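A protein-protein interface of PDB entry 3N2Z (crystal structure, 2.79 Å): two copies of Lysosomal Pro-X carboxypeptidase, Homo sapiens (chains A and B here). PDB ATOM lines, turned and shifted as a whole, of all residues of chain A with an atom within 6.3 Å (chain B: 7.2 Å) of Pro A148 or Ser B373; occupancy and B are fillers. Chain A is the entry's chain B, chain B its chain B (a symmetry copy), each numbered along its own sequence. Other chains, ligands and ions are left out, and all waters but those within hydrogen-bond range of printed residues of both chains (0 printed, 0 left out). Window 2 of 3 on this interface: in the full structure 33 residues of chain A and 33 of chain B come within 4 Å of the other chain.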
ATOM      1  N   PHE A 143     -12.496  26.641  -7.185  1.00  0.00           N
ATOM      2  CA  PHE A 143     -13.711  27.104  -6.518  1.00  0.00           C
ATOM      3  C   PHE A 143     -14.625  27.828  -7.540  1.00  0.00           C
ATOM      4  O   PHE A 143     -15.820  27.540  -7.568  1.00  0.00           O
ATOM      5  CB  PHE A 143     -13.393  27.958  -5.285  1.00  0.00           C
ATOM      6  CG  PHE A 143     -14.530  28.095  -4.299  1.00  0.00           C
ATOM      7  CD1 PHE A 143     -15.403  27.034  -4.064  1.00  0.00           C
ATOM      8  CD2 PHE A 143     -14.708  29.269  -3.581  1.00  0.00           C
ATOM      9  CE1 PHE A 143     -16.458  27.165  -3.156  1.00  0.00           C
ATOM     10  CE2 PHE A 143     -15.753  29.397  -2.669  1.00  0.00           C
ATOM     11  CZ  PHE A 143     -16.621  28.346  -2.458  1.00  0.00           C
ATOM     12  N   ARG A 144     -14.067  28.682  -8.439  1.00  0.00           N
ATOM     13  CA  ARG A 144     -14.904  29.288  -9.488  1.00  0.00           C
ATOM     14  C   ARG A 144     -15.359  28.233 -10.504  1.00  0.00           C
ATOM     15  O   ARG A 144     -16.501  28.293 -10.971  1.00  0.00           O
ATOM     16  CB  ARG A 144     -14.252  30.491 -10.197  1.00  0.00           C
ATOM     17  CG  ARG A 144     -14.894  30.775 -11.571  1.00  0.00           C
ATOM     18  CD  ARG A 144     -15.381  32.180 -11.747  1.00  0.00           C
ATOM     19  NE  ARG A 144     -16.758  32.380 -11.315  1.00  0.00           N
ATOM     20  CZ  ARG A 144     -17.772  32.677 -12.121  1.00  0.00           C
ATOM     21  NH1 ARG A 144     -18.981  32.877 -11.625  1.00  0.00           N
ATOM     22  NH2 ARG A 144     -17.579  32.788 -13.430  1.00  0.00           N
ATOM     23  N   MET A 145     -14.495  27.271 -10.831  1.00  0.00           N
ATOM     24  CA  MET A 145     -14.845  26.213 -11.789  1.00  0.00           C
ATOM     25  C   MET A 145     -16.034  25.337 -11.328  1.00  0.00           C
ATOM     26  O   MET A 145     -16.922  25.006 -12.130  1.00  0.00           O
ATOM     27  CB  MET A 145     -13.641  25.304 -12.065  1.00  0.00           C
ATOM     28  CG  MET A 145     -12.413  26.028 -12.590  1.00  0.00           C
ATOM     29  SD  MET A 145     -11.192  24.857 -13.235  1.00  0.00           S
ATOM     30  CE  MET A 145      -9.762  25.919 -13.317  1.00  0.00           C
ATOM     31  N   LYS A 146     -16.033  24.954 -10.033  1.00  0.00           N
ATOM     32  CA  LYS A 146     -17.051  24.068  -9.475  1.00  0.00           C
ATOM     33  C   LYS A 146     -18.203  24.802  -8.799  1.00  0.00           C
ATOM     34  O   LYS A 146     -19.350  24.352  -8.890  1.00  0.00           O
ATOM     35  CB  LYS A 146     -16.405  23.022  -8.543  1.00  0.00           C
ATOM     36  CG  LYS A 146     -15.381  22.094  -9.218  1.00  0.00           C
ATOM     37  CD  LYS A 146     -16.025  20.928  -9.920  1.00  0.00           C
ATOM     38  CE  LYS A 146     -14.992  20.036 -10.556  1.00  0.00           C
ATOM     39  NZ  LYS A 146     -15.605  18.846 -11.230  1.00  0.00           N
ATOM     40  N   TYR A 147     -17.919  25.924  -8.124  1.00  0.00           N
ATOM     41  CA  TYR A 147     -18.981  26.671  -7.464  1.00  0.00           C
ATOM     42  C   TYR A 147     -19.132  28.100  -8.070  1.00  0.00           C
ATOM     43  O   TYR A 147     -18.949  29.094  -7.346  1.00  0.00           O
ATOM     44  CB  TYR A 147     -18.767  26.676  -5.931  1.00  0.00           C
ATOM     45  CG  TYR A 147     -18.692  25.299  -5.292  1.00  0.00           C
ATOM     46  CD1 TYR A 147     -19.746  24.804  -4.525  1.00  0.00           C
ATOM     47  CD2 TYR A 147     -17.543  24.516  -5.405  1.00  0.00           C
ATOM     48  CE1 TYR A 147     -19.673  23.548  -3.917  1.00  0.00           C
ATOM     49  CE2 TYR A 147     -17.471  23.247  -4.829  1.00  0.00           C
ATOM     50  CZ  TYR A 147     -18.533  22.771  -4.072  1.00  0.00           C
ATOM     51  OH  TYR A 147     -18.453  21.523  -3.487  1.00  0.00           O
ATOM     52  N   PRO A 148     -19.483  28.246  -9.388  1.00  0.00           N
ATOM     53  CA  PRO A 148     -19.641  29.606  -9.945  1.00  0.00           C
ATOM     54  C   PRO A 148     -20.828  30.349  -9.311  1.00  0.00           C
ATOM     55  O   PRO A 148     -20.906  31.573  -9.365  1.00  0.00           O
ATOM     56  CB  PRO A 148     -19.807  29.367 -11.450  1.00  0.00           C
ATOM     57  CG  PRO A 148     -20.293  27.980 -11.574  1.00  0.00           C
ATOM     58  CD  PRO A 148     -19.761  27.215 -10.418  1.00  0.00           C
ATOM     59  N   HIS A 149     -21.734  29.606  -8.668  1.00  0.00           N
ATOM     60  CA  HIS A 149     -22.877  30.192  -7.968  1.00  0.00           C
ATOM     61  C   HIS A 149     -22.452  30.808  -6.638  1.00  0.00           C
ATOM     62  O   HIS A 149     -23.237  31.545  -6.071  1.00  0.00           O
ATOM     63  CB  HIS A 149     -23.971  29.156  -7.743  1.00  0.00           C
ATOM     64  CG  HIS A 149     -23.483  27.877  -7.147  1.00  0.00           C
ATOM     65  ND1 HIS A 149     -23.003  26.842  -7.947  1.00  0.00           N
ATOM     66  CD2 HIS A 149     -23.425  27.494  -5.852  1.00  0.00           C
ATOM     67  CE1 HIS A 149     -22.684  25.866  -7.115  1.00  0.00           C
ATOM     68  NE2 HIS A 149     -22.923  26.208  -5.844  1.00  0.00           N
ATOM     69  N   MET A 150     -21.228  30.525  -6.137  1.00  0.00           N
ATOM     70  CA  MET A 150     -20.737  31.081  -4.869  1.00  0.00           C
ATOM     71  C   MET A 150     -19.818  32.258  -5.086  1.00  0.00           C
ATOM     72  O   MET A 150     -19.858  33.200  -4.310  1.00  0.00           O
ATOM     73  CB  MET A 150     -19.979  30.037  -4.022  1.00  0.00           C
ATOM     74  CG  MET A 150     -20.794  28.828  -3.604  1.00  0.00           C
ATOM     75  SD  MET A 150     -22.369  29.097  -2.734  1.00  0.00           S
ATOM     76  CE  MET A 150     -21.858  29.988  -1.348  1.00  0.00           C
ATOM     77  N   VAL A 151     -18.939  32.182  -6.091  1.00  0.00           N
ATOM     78  CA  VAL A 151     -17.976  33.242  -6.365  1.00  0.00           C
ATOM     79  C   VAL A 151     -18.126  33.790  -7.798  1.00  0.00           C
ATOM     80  O   VAL A 151     -18.394  33.025  -8.740  1.00  0.00           O
ATOM     81  CB  VAL A 151     -16.523  32.849  -5.994  1.00  0.00           C
ATOM     82  CG1 VAL A 151     -16.356  32.667  -4.489  1.00  0.00           C
ATOM     83  CG2 VAL A 151     -16.048  31.621  -6.758  1.00  0.00           C
ATOM     84  N   VAL A 152     -17.988  35.124  -7.957  1.00  0.00           N
ATOM     85  CA  VAL A 152     -18.146  35.776  -9.288  1.00  0.00           C
ATOM     86  C   VAL A 152     -16.951  35.537 -10.164  1.00  0.00           C
ATOM     87  O   VAL A 152     -17.084  35.435 -11.386  1.00  0.00           O
ATOM     88  CB  VAL A 152     -18.534  37.284  -9.258  1.00  0.00           C
ATOM     89  CG1 VAL A 152     -19.963  37.466  -8.797  1.00  0.00           C
ATOM     90  CG2 VAL A 152     -17.586  38.102  -8.396  1.00  0.00           C
ATOM     91  N   SER A 373     -14.480  26.597 -21.147  1.00  0.00           N
ATOM     92  CA  SER A 373     -15.859  26.978 -20.843  1.00  0.00           C
ATOM     93  C   SER A 373     -16.008  27.866 -19.612  1.00  0.00           C
ATOM     94  O   SER A 373     -17.000  28.580 -19.518  1.00  0.00           O
ATOM     95  CB  SER A 373     -16.740  25.747 -20.726  1.00  0.00           C
ATOM     96  OG  SER A 373     -16.345  24.983 -19.602  1.00  0.00           O
ATOM     97  N   THR A 375     -15.158  30.988 -16.817  1.00  0.00           N
ATOM     98  CA  THR A 375     -15.030  32.435 -16.977  1.00  0.00           C
ATOM     99  C   THR A 375     -14.557  33.069 -15.679  1.00  0.00           C
ATOM    100  O   THR A 375     -14.635  32.462 -14.628  1.00  0.00           O
ATOM    101  CB  THR A 375     -16.426  33.062 -17.348  1.00  0.00           C
ATOM    102  OG1 THR A 375     -17.380  32.762 -16.325  1.00  0.00           O
ATOM    103  CG2 THR A 375     -16.980  32.608 -18.700  1.00  0.00           C
ATOM    104  N   MET B 145     -22.458  20.784 -15.862  1.00  0.00           N
ATOM    105  CA  MET B 145     -22.109  21.853 -14.915  1.00  0.00           C
ATOM    106  C   MET B 145     -20.763  21.616 -14.192  1.00  0.00           C
ATOM    107  O   MET B 145     -19.960  22.550 -14.032  1.00  0.00           O
ATOM    108  CB  MET B 145     -23.209  22.031 -13.862  1.00  0.00           C
ATOM    109  CG  MET B 145     -24.583  22.337 -14.432  1.00  0.00           C
ATOM    110  SD  MET B 145     -25.718  22.897 -13.137  1.00  0.00           S
ATOM    111  CE  MET B 145     -27.273  22.713 -13.990  1.00  0.00           C
ATOM    112  N   LYS B 146     -20.530  20.363 -13.745  1.00  0.00           N
ATOM    113  CA  LYS B 146     -19.336  20.008 -12.983  1.00  0.00           C
ATOM    114  C   LYS B 146     -18.208  19.440 -13.835  1.00  0.00           C
ATOM    115  O   LYS B 146     -17.035  19.713 -13.557  1.00  0.00           O
ATOM    116  CB  LYS B 146     -19.701  19.077 -11.809  1.00  0.00           C
ATOM    117  CG  LYS B 146     -20.678  19.675 -10.784  1.00  0.00           C
ATOM    118  CD  LYS B 146     -19.991  20.537  -9.758  1.00  0.00           C
ATOM    119  CE  LYS B 146     -20.976  21.092  -8.764  1.00  0.00           C
ATOM    120  NZ  LYS B 146     -20.312  21.924  -7.709  1.00  0.00           N
ATOM    121  N   MET B 365     -24.309  22.387  -3.681  1.00  0.00           N
ATOM    122  CA  MET B 365     -23.459  21.693  -4.631  1.00  0.00           C
ATOM    123  C   MET B 365     -23.697  22.165  -6.096  1.00  0.00           C
ATOM    124  O   MET B 365     -22.801  22.744  -6.717  1.00  0.00           O
ATOM    125  CB  MET B 365     -23.637  20.169  -4.467  1.00  0.00           C
ATOM    126  CG  MET B 365     -22.789  19.325  -5.412  1.00  0.00           C
ATOM    127  SD  MET B 365     -21.026  19.433  -5.039  1.00  0.00           S
ATOM    128  CE  MET B 365     -20.384  18.280  -6.228  1.00  0.00           C
ATOM    129  N   GLY B 367     -25.893  24.539  -7.354  1.00  0.00           N
ATOM    130  CA  GLY B 367     -26.204  25.954  -7.549  1.00  0.00           C
ATOM    131  C   GLY B 367     -27.598  26.518  -7.494  1.00  0.00           C
ATOM    132  O   GLY B 367     -27.745  27.754  -7.404  1.00  0.00           O
ATOM    133  N   ASN B 370     -29.115  29.719  -9.672  1.00  0.00           N
ATOM    134  CA  ASN B 370     -27.926  30.463 -10.065  1.00  0.00           C
ATOM    135  C   ASN B 370     -26.972  29.610 -10.923  1.00  0.00           C
ATOM    136  O   ASN B 370     -25.947  29.143 -10.431  1.00  0.00           O
ATOM    137  CB  ASN B 370     -27.256  30.982  -8.815  1.00  0.00           C
ATOM    138  CG  ASN B 370     -28.210  31.710  -7.905  1.00  0.00           C
ATOM    139  OD1 ASN B 370     -28.800  31.120  -6.998  1.00  0.00           O
ATOM    140  ND2 ASN B 370     -28.382  33.004  -8.131  1.00  0.00           N
ATOM    141  N   ILE B 371     -27.315  29.412 -12.214  1.00  0.00           N
ATOM    142  CA  ILE B 371     -26.558  28.588 -13.159  1.00  0.00           C
ATOM    143  C   ILE B 371     -26.303  29.273 -14.532  1.00  0.00           C
ATOM    144  O   ILE B 371     -25.975  28.599 -15.503  1.00  0.00           O
ATOM    145  CB  ILE B 371     -27.271  27.213 -13.322  1.00  0.00           C
ATOM    146  CG1 ILE B 371     -28.779  27.387 -13.694  1.00  0.00           C
ATOM    147  CG2 ILE B 371     -27.072  26.332 -12.073  1.00  0.00           C
ATOM    148  CD1 ILE B 371     -29.467  26.159 -14.307  1.00  0.00           C
ATOM    149  N   SER B 372     -26.442  30.602 -14.601  1.00  0.00           N
ATOM    150  CA  SER B 372     -26.278  31.405 -15.827  1.00  0.00           C
ATOM    151  C   SER B 372     -24.912  31.270 -16.514  1.00  0.00           C
ATOM    152  O   SER B 372     -24.846  31.369 -17.745  1.00  0.00           O
ATOM    153  CB  SER B 372     -26.611  32.877 -15.580  1.00  0.00           C
ATOM    154  OG  SER B 372     -26.787  33.166 -14.200  1.00  0.00           O
ATOM    155  N   SER B 373     -23.834  31.029 -15.734  1.00  0.00           N
ATOM    156  CA  SER B 373     -22.487  30.884 -16.288  1.00  0.00           C
ATOM    157  C   SER B 373     -22.286  29.623 -17.123  1.00  0.00           C
ATOM    158  O   SER B 373     -21.393  29.610 -17.963  1.00  0.00           O
ATOM    159  CB  SER B 373     -21.444  30.972 -15.190  1.00  0.00           C
ATOM    160  OG  SER B 373     -21.574  29.862 -14.319  1.00  0.00           O
ATOM    161  N   HIS B 374     -23.100  28.580 -16.915  1.00  0.00           N
ATOM    162  CA  HIS B 374     -22.985  27.329 -17.663  1.00  0.00           C
ATOM    163  C   HIS B 374     -23.462  27.488 -19.090  1.00  0.00           C
ATOM    164  O   HIS B 374     -24.086  28.489 -19.426  1.00  0.00           O
ATOM    165  CB  HIS B 374     -23.679  26.144 -16.948  1.00  0.00           C
ATOM    166  CG  HIS B 374     -23.237  25.966 -15.524  1.00  0.00           C
ATOM    167  ND1 HIS B 374     -21.992  25.454 -15.210  1.00  0.00           N
ATOM    168  CD2 HIS B 374     -23.886  26.273 -14.376  1.00  0.00           C
ATOM    169  CE1 HIS B 374     -21.929  25.466 -13.892  1.00  0.00           C
ATOM    170  NE2 HIS B 374     -23.046  25.960 -13.350  1.00  0.00           N
ATOM    171  N   THR B 375     -23.139  26.525 -19.944  1.00  0.00           N
ATOM    172  CA  THR B 375     -23.478  26.564 -21.365  1.00  0.00           C
ATOM    173  C   THR B 375     -23.844  25.173 -21.857  1.00  0.00           C
ATOM    174  O   THR B 375     -23.539  24.187 -21.213  1.00  0.00           O
ATOM    175  CB  THR B 375     -22.244  27.069 -22.201  1.00  0.00           C
ATOM    176  OG1 THR B 375     -21.125  26.206 -21.984  1.00  0.00           O
ATOM    177  CG2 THR B 375     -21.831  28.512 -21.900  1.00  0.00           C
ATOM    178  N   ILE B 396     -32.530  30.438 -19.891  1.00  0.00           N
ATOM    179  CA  ILE B 396     -31.706  31.183 -18.930  1.00  0.00           C
ATOM    180  C   ILE B 396     -30.756  32.073 -19.762  1.00  0.00           C
ATOM    181  O   ILE B 396     -30.541  33.235 -19.418  1.00  0.00           O
ATOM    182  CB  ILE B 396     -30.961  30.277 -17.910  1.00  0.00           C
ATOM    183  CG1 ILE B 396     -31.934  29.424 -17.090  1.00  0.00           C
ATOM    184  CG2 ILE B 396     -30.087  31.098 -16.976  1.00  0.00           C
ATOM    185  CD1 ILE B 396     -31.973  27.982 -17.487  1.00  0.00           C
ATOM    186  N   THR B 397     -30.198  31.516 -20.857  1.00  0.00           N
ATOM    187  CA  THR B 397     -29.288  32.187 -21.787  1.00  0.00           C
ATOM    188  C   THR B 397     -29.595  31.638 -23.189  1.00  0.00           C
ATOM    189  O   THR B 397     -30.552  30.887 -23.365  1.00  0.00           O
ATOM    190  CB  THR B 397     -27.797  31.927 -21.408  1.00  0.00           C
ATOM    191  OG1 THR B 397     -27.480  30.535 -21.557  1.00  0.00           O
ATOM    192  CG2 THR B 397     -27.428  32.411 -20.020  1.00  0.00           C
ATOM    193  N   THR B 399     -27.670  29.621 -24.732  1.00  0.00           N
ATOM    194  CA  THR B 399     -27.052  28.304 -24.643  1.00  0.00           C
ATOM    195  C   THR B 399     -27.691  27.389 -23.576  1.00  0.00           C
ATOM    196  O   THR B 399     -27.643  26.163 -23.721  1.00  0.00           O
ATOM    197  CB  THR B 399     -25.522  28.470 -24.663  1.00  0.00           C
ATOM    198  OG1 THR B 399     -24.929  27.197 -24.566  1.00  0.00           O
ATOM    199  CG2 THR B 399     -24.996  29.387 -23.549  1.00  0.00           C
ATOM    200  N   LEU B 400     -28.309  27.986 -22.522  1.00  0.00           N
ATOM    201  CA  LEU B 400     -29.052  27.251 -21.473  1.00  0.00           C
ATOM    202  C   LEU B 400     -30.518  27.507 -21.850  1.00  0.00           C
ATOM    203  O   LEU B 400     -31.114  28.539 -21.512  1.00  0.00           O
ATOM    204  CB  LEU B 400     -28.732  27.777 -20.068  1.00  0.00           C
ATOM    205  CG  LEU B 400     -27.326  27.575 -19.548  1.00  0.00           C
ATOM    206  CD1 LEU B 400     -27.181  28.270 -18.260  1.00  0.00           C
ATOM    207  CD2 LEU B 400     -27.006  26.115 -19.389  1.00  0.00           C
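Among the printed residues, merely in contact across the chains: His A149 with Met B365 (3.1 Å), His A149 with Asn B370 (3.3 Å), His A149 with Gly B367 (3.3 Å), Pro A148 with Ser B373 (3.4 Å) and Pro A148 with His B374 (3.8 Å).
Lys B146 touches its own counterpart, Lys A146. 4 positions are printed for both chains. Of the 7 pairs that touch across the chains among the printed residues, 1 has its exchanged pair printed and touching as well.
NH1 of Arg A144 is in hydrogen-bond range of O of Pro A148, at 3.2 Å. The side-chain amino group (NZ) of Lys B146 lies within hydrogen-bond range of the backbone carbonyl oxygen (O) of Met B365, at 2.8 Å.
Of the 12 printed residues of chain A, 4 touch a printed residue of chain B. Hydrophobic or aromatic side chains of chain A within 4 Å of the printed part of chain B: Tyr A147, Pro A148 and His A149. Hydrophobic or aromatic side chains of chain B within 4 Å of the printed part of chain A: Met B365 and His B374. Among the printed residues, 7 pairs touch across the chains.
Of the printed residues of chain B, Lys A146 touches Lys B146. Of the printed residues of chain B, Tyr A147 touches Met B365. Of chain B, only Ser B373 and His B374 come within 4 Å of Pro A148. Of the printed residues of chain B, His A149 touches Met B365, Gly B367 and Asn B370. Thr A375 touches none of the printed residues of chain B. Printed residues of chain A within 4 Å of Gly B367: His A149. Of the printed residues of chain A, Asn B370 touches His A149. Ser B373 touches just one residue of chain A: Pro A148 (3.4 Å). The nearest residue of chain A that does not touch Ser B373 is Thr A375 (4.6 Å).
The side-chain amino group (NZ) of Lys A146 lies within hydrogen-bond range of the backbone carbonyl oxygen (O) of Lys B146 (2.9 Å). The side-chain hydroxyl (OH) of Tyr A147 lies within hydrogen-bond range of the side-chain sulfur (SD) of Met B365, at 3.7 Å.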
